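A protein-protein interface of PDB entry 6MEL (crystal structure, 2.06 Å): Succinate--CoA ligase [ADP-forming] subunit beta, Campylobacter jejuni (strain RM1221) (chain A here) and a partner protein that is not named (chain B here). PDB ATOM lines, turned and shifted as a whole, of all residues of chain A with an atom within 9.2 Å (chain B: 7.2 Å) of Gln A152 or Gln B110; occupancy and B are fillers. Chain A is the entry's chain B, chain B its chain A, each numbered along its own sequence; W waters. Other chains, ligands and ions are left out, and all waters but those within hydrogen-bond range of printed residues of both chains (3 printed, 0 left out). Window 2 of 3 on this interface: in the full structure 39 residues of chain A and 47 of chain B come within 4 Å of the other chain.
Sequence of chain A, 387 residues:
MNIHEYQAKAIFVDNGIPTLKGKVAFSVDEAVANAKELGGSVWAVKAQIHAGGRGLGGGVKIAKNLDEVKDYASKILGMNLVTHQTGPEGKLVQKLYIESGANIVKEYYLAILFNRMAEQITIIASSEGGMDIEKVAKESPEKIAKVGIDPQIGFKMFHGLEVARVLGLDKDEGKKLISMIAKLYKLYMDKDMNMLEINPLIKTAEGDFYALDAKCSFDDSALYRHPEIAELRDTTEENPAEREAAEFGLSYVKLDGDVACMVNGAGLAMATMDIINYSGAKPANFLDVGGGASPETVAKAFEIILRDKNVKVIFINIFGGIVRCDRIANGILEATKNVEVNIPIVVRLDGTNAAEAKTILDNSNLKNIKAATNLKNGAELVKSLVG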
ATOM      1  N   ALA A 118       3.772  13.932   0.771  1.00  0.00           N
ATOM      2  CA  ALA A 118       5.249  14.028   0.675  1.00  0.00           C
ATOM      3  C   ALA A 118       5.930  13.161   1.740  1.00  0.00           C
ATOM      4  O   ALA A 118       7.148  13.076   1.787  1.00  0.00           O
ATOM      5  CB  ALA A 118       5.662  15.476   0.797  1.00  0.00           C
ATOM      6  N   GLU A 119       5.143  12.559   2.648  1.00  0.00           N
ATOM      7  CA  GLU A 119       5.625  11.782   3.788  1.00  0.00           C
ATOM      8  C   GLU A 119       6.594  12.644   4.601  1.00  0.00           C
ATOM      9  O   GLU A 119       7.696  12.181   5.004  1.00  0.00           O
ATOM     10  CB  GLU A 119       6.350  10.501   3.335  1.00  0.00           C
ATOM     11  CG  GLU A 119       5.474   9.524   2.592  1.00  0.00           C
ATOM     12  CD  GLU A 119       6.241   8.283   2.138  1.00  0.00           C
ATOM     13  OE1 GLU A 119       7.415   8.154   2.477  1.00  0.00           O
ATOM     14  OE2 GLU A 119       5.683   7.467   1.427  1.00  0.00           O
ATOM     15  N   GLN A 120       6.231  13.901   4.835  1.00  0.00           N
ATOM     16  CA  GLN A 120       7.121  14.754   5.650  1.00  0.00           C
ATOM     17  C   GLN A 120       6.272  15.765   6.424  1.00  0.00           C
ATOM     18  O   GLN A 120       5.095  15.546   6.549  1.00  0.00           O
ATOM     19  CB  GLN A 120       8.167  15.393   4.744  1.00  0.00           C
ATOM     20  CG  GLN A 120       7.559  16.403   3.829  1.00  0.00           C
ATOM     21  CD  GLN A 120       8.580  17.131   2.980  1.00  0.00           C
ATOM     22  OE1 GLN A 120       9.711  16.636   2.778  1.00  0.00           O
ATOM     23  NE2 GLN A 120       8.133  18.296   2.480  1.00  0.00           N
ATOM     24  N   ILE A 121       6.921  16.754   7.072  1.00  0.00           N
ATOM     25  CA  ILE A 121       6.243  17.705   7.897  1.00  0.00           C
ATOM     26  C   ILE A 121       6.129  19.010   7.085  1.00  0.00           C
ATOM     27  O   ILE A 121       6.978  19.308   6.208  1.00  0.00           O
ATOM     28  CB  ILE A 121       6.954  17.836   9.256  1.00  0.00           C
ATOM     29  CG1 ILE A 121       6.669  16.607  10.117  1.00  0.00           C
ATOM     30  CG2 ILE A 121       6.507  19.073  10.002  1.00  0.00           C
ATOM     31  CD1 ILE A 121       7.760  15.661  10.219  1.00  0.00           C
ATOM     32  N   ILE A 149       9.458  20.288   5.530  1.00  0.00           N
ATOM     33  CA  ILE A 149      10.531  19.912   6.410  1.00  0.00           C
ATOM     34  C   ILE A 149      10.771  18.398   6.275  1.00  0.00           C
ATOM     35  O   ILE A 149       9.950  17.579   6.721  1.00  0.00           O
ATOM     36  CB  ILE A 149      10.204  20.219   7.876  1.00  0.00           C
ATOM     37  CG1 ILE A 149       9.682  21.644   8.118  1.00  0.00           C
ATOM     38  CG2 ILE A 149      11.404  19.879   8.742  1.00  0.00           C
ATOM     39  CD1 ILE A 149      10.620  22.730   7.683  1.00  0.00           C
ATOM     40  N   ASP A 150      11.882  18.030   5.661  1.00  0.00           N
ATOM     41  CA  ASP A 150      12.286  16.632   5.605  1.00  0.00           C
ATOM     42  C   ASP A 150      12.771  16.245   7.008  1.00  0.00           C
ATOM     43  O   ASP A 150      13.710  16.833   7.554  1.00  0.00           O
ATOM     44  CB  ASP A 150      13.280  16.400   4.463  1.00  0.00           C
ATOM     45  CG  ASP A 150      13.716  14.959   4.294  1.00  0.00           C
ATOM     46  OD1 ASP A 150      13.648  14.177   5.302  1.00  0.00           O
ATOM     47  OD2 ASP A 150      14.154  14.620   3.177  1.00  0.00           O
ATOM     48  N   PRO A 151      12.111  15.271   7.664  1.00  0.00           N
ATOM     49  CA  PRO A 151      12.462  14.916   9.030  1.00  0.00           C
ATOM     50  C   PRO A 151      13.865  14.324   9.190  1.00  0.00           C
ATOM     51  O   PRO A 151      14.353  14.240  10.301  1.00  0.00           O
ATOM     52  CB  PRO A 151      11.395  13.881   9.402  1.00  0.00           C
ATOM     53  CG  PRO A 151      10.989  13.272   8.074  1.00  0.00           C
ATOM     54  CD  PRO A 151      11.038  14.425   7.099  1.00  0.00           C
ATOM     55  N   GLN A 152      14.515  13.950   8.089  1.00  0.00           N
ATOM     56  CA  GLN A 152      15.858  13.497   8.135  1.00  0.00           C
ATOM     57  C   GLN A 152      16.737  14.629   8.663  1.00  0.00           C
ATOM     58  O   GLN A 152      17.722  14.356   9.344  1.00  0.00           O
ATOM     59  CB  GLN A 152      16.343  13.066   6.751  1.00  0.00           C
ATOM     60  CG  GLN A 152      17.790  12.591   6.743  1.00  0.00           C
ATOM     61  CD  GLN A 152      18.195  11.910   5.439  1.00  0.00           C
ATOM     62  OE1 GLN A 152      17.369  11.452   4.646  1.00  0.00           O
ATOM     63  NE2 GLN A 152      19.494  11.795   5.213  1.00  0.00           N
ATOM     64  N   ILE A 153      16.443  15.871   8.262  1.00  0.00           N
ATOM     65  CA  ILE A 153      17.255  17.016   8.677  1.00  0.00           C
ATOM     66  C   ILE A 153      16.545  17.804   9.783  1.00  0.00           C
ATOM     67  O   ILE A 153      17.176  18.566  10.543  1.00  0.00           O
ATOM     68  CB  ILE A 153      17.637  17.950   7.497  1.00  0.00           C
ATOM     69  CG1 ILE A 153      16.446  18.505   6.717  1.00  0.00           C
ATOM     70  CG2 ILE A 153      18.606  17.228   6.560  1.00  0.00           C
ATOM     71  CD1 ILE A 153      16.789  19.641   5.789  1.00  0.00           C
ATOM     72  N   GLY A 154      15.215  17.742   9.822  1.00  0.00           N
ATOM     73  CA  GLY A 154      14.465  18.608  10.774  1.00  0.00           C
ATOM     74  C   GLY A 154      14.481  20.085  10.396  1.00  0.00           C
ATOM     75  O   GLY A 154      14.947  20.477   9.320  1.00  0.00           O
ATOM     76  N   PHE A 155      13.929  20.907  11.300  1.00  0.00           N
ATOM     77  CA  PHE A 155      13.758  22.344  11.095  1.00  0.00           C
ATOM     78  C   PHE A 155      15.119  23.042  11.211  1.00  0.00           C
ATOM     79  O   PHE A 155      15.906  22.761  12.082  1.00  0.00           O
ATOM     80  CB  PHE A 155      12.769  22.905  12.111  1.00  0.00           C
ATOM     81  CG  PHE A 155      12.659  24.398  12.077  1.00  0.00           C
ATOM     82  CD1 PHE A 155      11.945  25.011  11.075  1.00  0.00           C
ATOM     83  CD2 PHE A 155      13.296  25.185  13.018  1.00  0.00           C
ATOM     84  CE1 PHE A 155      11.827  26.392  11.032  1.00  0.00           C
ATOM     85  CE2 PHE A 155      13.140  26.568  12.992  1.00  0.00           C
ATOM     86  CZ  PHE A 155      12.420  27.161  11.995  1.00  0.00           C
ATOM     87  N   LYS A 156      15.442  23.847  10.206  1.00  0.00           N
ATOM     88  CA  LYS A 156      16.763  24.503  10.107  1.00  0.00           C
ATOM     89  C   LYS A 156      16.523  26.021  10.004  1.00  0.00           C
ATOM     90  O   LYS A 156      15.471  26.449   9.555  1.00  0.00           O
ATOM     91  CB  LYS A 156      17.489  23.948   8.875  1.00  0.00           C
ATOM     92  CG  LYS A 156      17.965  22.509   9.011  1.00  0.00           C
ATOM     93  CD  LYS A 156      19.094  22.404   9.997  1.00  0.00           C
ATOM     94  CE  LYS A 156      20.036  21.285   9.680  1.00  0.00           C
ATOM     95  NZ  LYS A 156      20.942  21.049  10.821  1.00  0.00           N
ATOM     96  N   HIS A 159      14.919  27.253   6.836  1.00  0.00           N
ATOM     97  CA  HIS A 159      13.438  27.110   6.810  1.00  0.00           C
ATOM     98  C   HIS A 159      12.823  28.314   7.521  1.00  0.00           C
ATOM     99  O   HIS A 159      11.882  28.918   7.047  1.00  0.00           O
ATOM    100  CB  HIS A 159      12.979  25.814   7.496  1.00  0.00           C
ATOM    101  CG  HIS A 159      13.409  24.523   6.866  1.00  0.00           C
ATOM    102  ND1 HIS A 159      14.051  23.545   7.590  1.00  0.00           N
ATOM    103  CD2 HIS A 159      13.183  23.997   5.642  1.00  0.00           C
ATOM    104  CE1 HIS A 159      14.241  22.491   6.811  1.00  0.00           C
ATOM    105  NE2 HIS A 159      13.694  22.724   5.623  1.00  0.00           N
ATOM    106  N   TYR A 185       8.869  22.546  16.769  1.00  0.00           N
ATOM    107  CA  TYR A 185       9.120  21.410  15.875  1.00  0.00           C
ATOM    108  C   TYR A 185       9.594  20.216  16.714  1.00  0.00           C
ATOM    109  O   TYR A 185       9.138  19.068  16.535  1.00  0.00           O
ATOM    110  CB  TYR A 185      10.126  21.738  14.774  1.00  0.00           C
ATOM    111  CG  TYR A 185      10.435  20.547  13.906  1.00  0.00           C
ATOM    112  CD1 TYR A 185       9.619  20.195  12.839  1.00  0.00           C
ATOM    113  CD2 TYR A 185      11.544  19.752  14.162  1.00  0.00           C
ATOM    114  CE1 TYR A 185       9.904  19.091  12.047  1.00  0.00           C
ATOM    115  CE2 TYR A 185      11.851  18.660  13.365  1.00  0.00           C
ATOM    116  CZ  TYR A 185      11.011  18.318  12.325  1.00  0.00           C
ATOM    117  OH  TYR A 185      11.298  17.237  11.555  1.00  0.00           O
ATOM    118  N   MET A 189       7.653  16.527  17.135  1.00  0.00           N
ATOM    119  CA  MET A 189       8.320  15.254  16.903  1.00  0.00           C
ATOM    120  C   MET A 189       8.339  14.411  18.185  1.00  0.00           C
ATOM    121  O   MET A 189       7.941  13.249  18.139  1.00  0.00           O
ATOM    122  CB  MET A 189       9.746  15.451  16.380  1.00  0.00           C
ATOM    123  CG  MET A 189       9.776  16.170  15.005  1.00  0.00           C
ATOM    124  SD  MET A 189       8.754  15.366  13.691  1.00  0.00           S
ATOM    125  CE  MET A 189       9.786  13.943  13.336  1.00  0.00           C
ATOM    126  N   ASP B 104       7.074   6.502  13.301  1.00  0.00           N
ATOM    127  CA  ASP B 104       8.028   5.366  13.242  1.00  0.00           C
ATOM    128  C   ASP B 104       8.091   4.847  11.810  1.00  0.00           C
ATOM    129  O   ASP B 104       9.152   4.502  11.298  1.00  0.00           O
ATOM    130  CB  ASP B 104       7.668   4.219  14.188  1.00  0.00           C
ATOM    131  CG  ASP B 104       7.811   4.511  15.665  1.00  0.00           C
ATOM    132  OD1 ASP B 104       8.372   5.584  16.034  1.00  0.00           O
ATOM    133  OD2 ASP B 104       7.360   3.643  16.453  1.00  0.00           O
ATOM    134  N   MET B 105       6.938   4.803  11.160  1.00  0.00           N
ATOM    135  CA  MET B 105       6.875   4.344   9.806  1.00  0.00           C
ATOM    136  C   MET B 105       7.553   5.345   8.865  1.00  0.00           C
ATOM    137  O   MET B 105       8.227   4.968   7.904  1.00  0.00           O
ATOM    138  CB  MET B 105       5.411   4.127   9.414  1.00  0.00           C
ATOM    139  CG  MET B 105       5.250   3.295   8.228  1.00  0.00           C
ATOM    140  SD  MET B 105       6.101   1.675   8.422  1.00  0.00           S
ATOM    141  CE  MET B 105       6.519   1.846   6.711  1.00  0.00           C
ATOM    142  N   MET B 106       7.388   6.642   9.149  1.00  0.00           N
ATOM    143  CA  MET B 106       8.004   7.670   8.341  1.00  0.00           C
ATOM    144  C   MET B 106       9.534   7.459   8.305  1.00  0.00           C
ATOM    145  O   MET B 106      10.153   7.454   7.236  1.00  0.00           O
ATOM    146  CB  MET B 106       7.684   9.061   8.900  1.00  0.00           C
ATOM    147  CG  MET B 106       8.075  10.222   7.981  1.00  0.00           C
ATOM    148  SD  MET B 106       7.548  11.850   8.654  1.00  0.00           S
ATOM    149  CE  MET B 106       8.350  11.797  10.243  1.00  0.00           C
ATOM    150  N   PHE B 107      10.152   7.358   9.477  1.00  0.00           N
ATOM    151  CA  PHE B 107      11.606   7.176   9.587  1.00  0.00           C
ATOM    152  C   PHE B 107      12.042   5.803   9.049  1.00  0.00           C
ATOM    153  O   PHE B 107      13.046   5.714   8.329  1.00  0.00           O
ATOM    154  CB  PHE B 107      12.092   7.359  11.024  1.00  0.00           C
ATOM    155  CG  PHE B 107      12.230   8.805  11.424  1.00  0.00           C
ATOM    156  CD1 PHE B 107      13.230   9.594  10.867  1.00  0.00           C
ATOM    157  CD2 PHE B 107      11.357   9.378  12.336  1.00  0.00           C
ATOM    158  CE1 PHE B 107      13.336  10.934  11.201  1.00  0.00           C
ATOM    159  CE2 PHE B 107      11.487  10.716  12.693  1.00  0.00           C
ATOM    160  CZ  PHE B 107      12.500  11.480  12.150  1.00  0.00           C
ATOM    161  N   ALA B 108      11.263   4.756   9.313  1.00  0.00           N
ATOM    162  CA  ALA B 108      11.663   3.411   8.865  1.00  0.00           C
ATOM    163  C   ALA B 108      11.622   3.320   7.336  1.00  0.00           C
ATOM    164  O   ALA B 108      12.512   2.736   6.737  1.00  0.00           O
ATOM    165  CB  ALA B 108      10.832   2.334   9.497  1.00  0.00           C
ATOM    166  N   LYS B 109      10.627   3.931   6.707  1.00  0.00           N
ATOM    167  CA  LYS B 109      10.562   3.944   5.270  1.00  0.00           C
ATOM    168  C   LYS B 109      11.733   4.718   4.634  1.00  0.00           C
ATOM    169  O   LYS B 109      12.229   4.294   3.605  1.00  0.00           O
ATOM    170  CB  LYS B 109       9.236   4.505   4.750  1.00  0.00           C
ATOM    171  CG  LYS B 109       9.131   4.423   3.229  1.00  0.00           C
ATOM    172  CD  LYS B 109       7.749   4.484   2.709  1.00  0.00           C
ATOM    173  CE  LYS B 109       7.649   4.486   1.207  1.00  0.00           C
ATOM    174  NZ  LYS B 109       6.363   5.062   0.821  1.00  0.00           N
ATOM    175  N   GLN B 110      12.115   5.864   5.202  1.00  0.00           N
ATOM    176  CA  GLN B 110      13.237   6.623   4.652  1.00  0.00           C
ATOM    177  C   GLN B 110      14.484   5.723   4.684  1.00  0.00           C
ATOM    178  O   GLN B 110      15.247   5.665   3.729  1.00  0.00           O
ATOM    179  CB  GLN B 110      13.522   7.909   5.438  1.00  0.00           C
ATOM    180  CG  GLN B 110      12.553   9.057   5.187  1.00  0.00           C
ATOM    181  CD  GLN B 110      13.208  10.379   5.530  1.00  0.00           C
ATOM    182  OE1 GLN B 110      14.327  10.425   6.037  1.00  0.00           O
ATOM    183  NE2 GLN B 110      12.533  11.475   5.226  1.00  0.00           N
ATOM    184  N   TYR B 111      14.657   4.947   5.759  1.00  0.00           N
ATOM    185  CA  TYR B 111      15.842   4.083   5.844  1.00  0.00           C
ATOM    186  C   TYR B 111      15.734   2.929   4.835  1.00  0.00           C
ATOM    187  O   TYR B 111      16.686   2.605   4.127  1.00  0.00           O
ATOM    188  CB  TYR B 111      16.096   3.617   7.275  1.00  0.00           C
ATOM    189  CG  TYR B 111      17.435   2.935   7.428  1.00  0.00           C
ATOM    190  CD1 TYR B 111      18.620   3.636   7.228  1.00  0.00           C
ATOM    191  CD2 TYR B 111      17.539   1.606   7.774  1.00  0.00           C
ATOM    192  CE1 TYR B 111      19.856   3.028   7.331  1.00  0.00           C
ATOM    193  CE2 TYR B 111      18.778   0.990   7.931  1.00  0.00           C
ATOM    194  CZ  TYR B 111      19.945   1.697   7.698  1.00  0.00           C
ATOM    195  OH  TYR B 111      21.186   1.150   7.875  1.00  0.00           O
ATOM    196  N   ALA B 112      14.562   2.303   4.759  1.00  0.00           N
ATOM    197  CA  ALA B 112      14.315   1.250   3.782  1.00  0.00           C
ATOM    198  C   ALA B 112      14.601   1.760   2.364  1.00  0.00           C
ATOM    199  O   ALA B 112      15.278   1.093   1.602  1.00  0.00           O
ATOM    200  CB  ALA B 112      12.916   0.751   3.910  1.00  0.00           C
ATOM    201  N   ASN B 113      14.105   2.958   2.037  1.00  0.00           N
ATOM    202  CA  ASN B 113      14.354   3.548   0.717  1.00  0.00           C
ATOM    203  C   ASN B 113      15.848   3.644   0.454  1.00  0.00           C
ATOM    204  O   ASN B 113      16.292   3.280  -0.601  1.00  0.00           O
ATOM    205  CB  ASN B 113      13.741   4.942   0.573  1.00  0.00           C
ATOM    206  CG  ASN B 113      12.220   4.939   0.537  1.00  0.00           C
ATOM    207  OD1 ASN B 113      11.586   3.919   0.301  1.00  0.00           O
ATOM    208  ND2 ASN B 113      11.635   6.105   0.715  1.00  0.00           N
ATOM    209  N   LYS B 114      16.612   4.151   1.419  1.00  0.00           N
ATOM    210  CA  LYS B 114      18.016   4.342   1.206  1.00  0.00           C
ATOM    211  C   LYS B 114      18.702   2.985   1.009  1.00  0.00           C
ATOM    212  O   LYS B 114      19.588   2.857   0.192  1.00  0.00           O
ATOM    213  CB  LYS B 114      18.688   5.037   2.387  1.00  0.00           C
ATOM    214  CG  LYS B 114      20.199   5.131   2.197  1.00  0.00           C
ATOM    215  CD  LYS B 114      20.899   6.001   3.184  1.00  0.00           C
ATOM    216  CE  LYS B 114      21.346   5.256   4.398  1.00  0.00           C
ATOM    217  NZ  LYS B 114      22.219   6.103   5.228  1.00  0.00           N
ATOM    218  N   LYS B 115      18.294   1.966   1.751  1.00  0.00           N
ATOM    219  CA  LYS B 115      18.961   0.648   1.618  1.00  0.00           C
ATOM    220  C   LYS B 115      18.452  -0.155   0.408  1.00  0.00           C
ATOM    221  O   LYS B 115      18.969  -1.216   0.152  1.00  0.00           O
ATOM    222  CB  LYS B 115      18.768  -0.164   2.901  1.00  0.00           C
ATOM    223  CG  LYS B 115      19.276   0.548   4.154  1.00  0.00           C
ATOM    224  CD  LYS B 115      20.742   0.918   4.116  1.00  0.00           C
ATOM    225  CE  LYS B 115      21.612  -0.294   3.829  1.00  0.00           C
ATOM    226  NZ  LYS B 115      23.030   0.095   3.907  1.00  0.00           N
ATOM    227  N   GLY B 116      17.420   0.321  -0.299  1.00  0.00           N
ATOM    228  CA  GLY B 116      16.823  -0.433  -1.438  1.00  0.00           C
ATOM    229  C   GLY B 116      15.854  -1.528  -0.995  1.00  0.00           C
ATOM    230  O   GLY B 116      15.647  -2.449  -1.711  1.00  0.00           O
ATOM    231  N   ILE B 119       8.744  -2.211   0.914  1.00  0.00           N
ATOM    232  CA  ILE B 119       7.823  -2.583   1.983  1.00  0.00           C
ATOM    233  C   ILE B 119       6.439  -2.826   1.387  1.00  0.00           C
ATOM    234  O   ILE B 119       5.998  -2.118   0.467  1.00  0.00           O
ATOM    235  CB  ILE B 119       7.770  -1.452   3.030  1.00  0.00           C
ATOM    236  CG1 ILE B 119       9.095  -1.239   3.758  1.00  0.00           C
ATOM    237  CG2 ILE B 119       6.627  -1.662   4.011  1.00  0.00           C
ATOM    238  CD1 ILE B 119       9.242   0.150   4.340  1.00  0.00           C
HETATM  239  O   HOH W   1       9.141   8.385   4.756  1.00  0.00           O
HETATM  240  O   HOH W   2       9.849  10.905   4.579  1.00  0.00           O
HETATM  241  O   HOH W   3       8.975   7.436   0.589  1.00  0.00           O
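Hydrophobic or aromatic side chains of chain A that line the printed part of chain B: Ile A121, Pro A151 and Met A189. Along chain A the printed residues that touch a printed residue of chain B span positions 119 to 189. Of the 14 printed residues of chain B, 4 touch a printed residue of chain A. Printed residues of chain B that touch a printed residue of chain A: Met B106, Phe B107, Lys B109 and Gln B110. Hydrophobic or aromatic side chains of chain B within 4 Å of the printed part of chain A: Met B106 and Phe B107. Among the printed residues, 9 pairs touch across the chains. Among the printed residues, Asp or Glu carboxylates within 4 Å of a Lys or Arg side-chain nitrogen of the other chain: Glu A119 with Lys B109.
The backbone carbonyl oxygen of Lys B109 sits close to the side-chain amide oxygen of Asn B113 (3.4 Å). The backbone NH (N) of Ile A149 is in hydrogen-bond range of the backbone carbonyl oxygen (O) of Ile A121, 2.8 Å away. OD1 of Asp A150 sits at hydrogen-bond distance from N of Gln A152, 2.9 Å away.
Printed residues of chain B within 4 Å of Glu A119: Met B106 (3.6 Å) and Lys B109 (2.6 Å). Of chain B, only Gln B110 (3.4 Å) comes within 4 Å of Gln A152. Of the printed residues of chain A, Met B106 touches Glu A119 (3.6 Å), Ile A121 (3.9 Å) and Pro A151 (3.7 Å). The nearest printed residue of chain B that does not touch Ile A121 is Phe B107 (6.6 Å).
Ile A121 touches Met B106 (CD1 to CE, 3.9 Å). Pro A151 touches Met B106. CE1 of Phe B107 touches O of Pro A151 (3.6 Å). CG of Pro A151 touches NE2 of Gln B110, at 3.7 Å. CE of Met A189 touches CE2 of Phe B107, at 3.7 Å.
The side-chain carboxylate of Glu A119 lies within salt-bridge range of the side-chain amino group of Lys B109 (2.6 Å). NE2 of Gln B110 lies within hydrogen-bond range of OD1 of Asp A150 (2.9 Å). OE1 of Gln B110 lies close to OE1 of Gln A152 (3.5 Å). SD of Met B106 lies close to O of Glu A119 (3.7 Å).
Water W2 lies within hydrogen-bond range of the backbone carbonyl oxygen of Glu A119 and the side-chain amide nitrogen of Gln B110. Water W3 bridges OE1 of Glu A119 (2.6 Å) and ND2 of Asn B113 (3.0 Å). Water W1 lies within hydrogen-bond range of O of Met B106 (2.8 Å) and OE1 of Glu A119 (2.9 Å).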
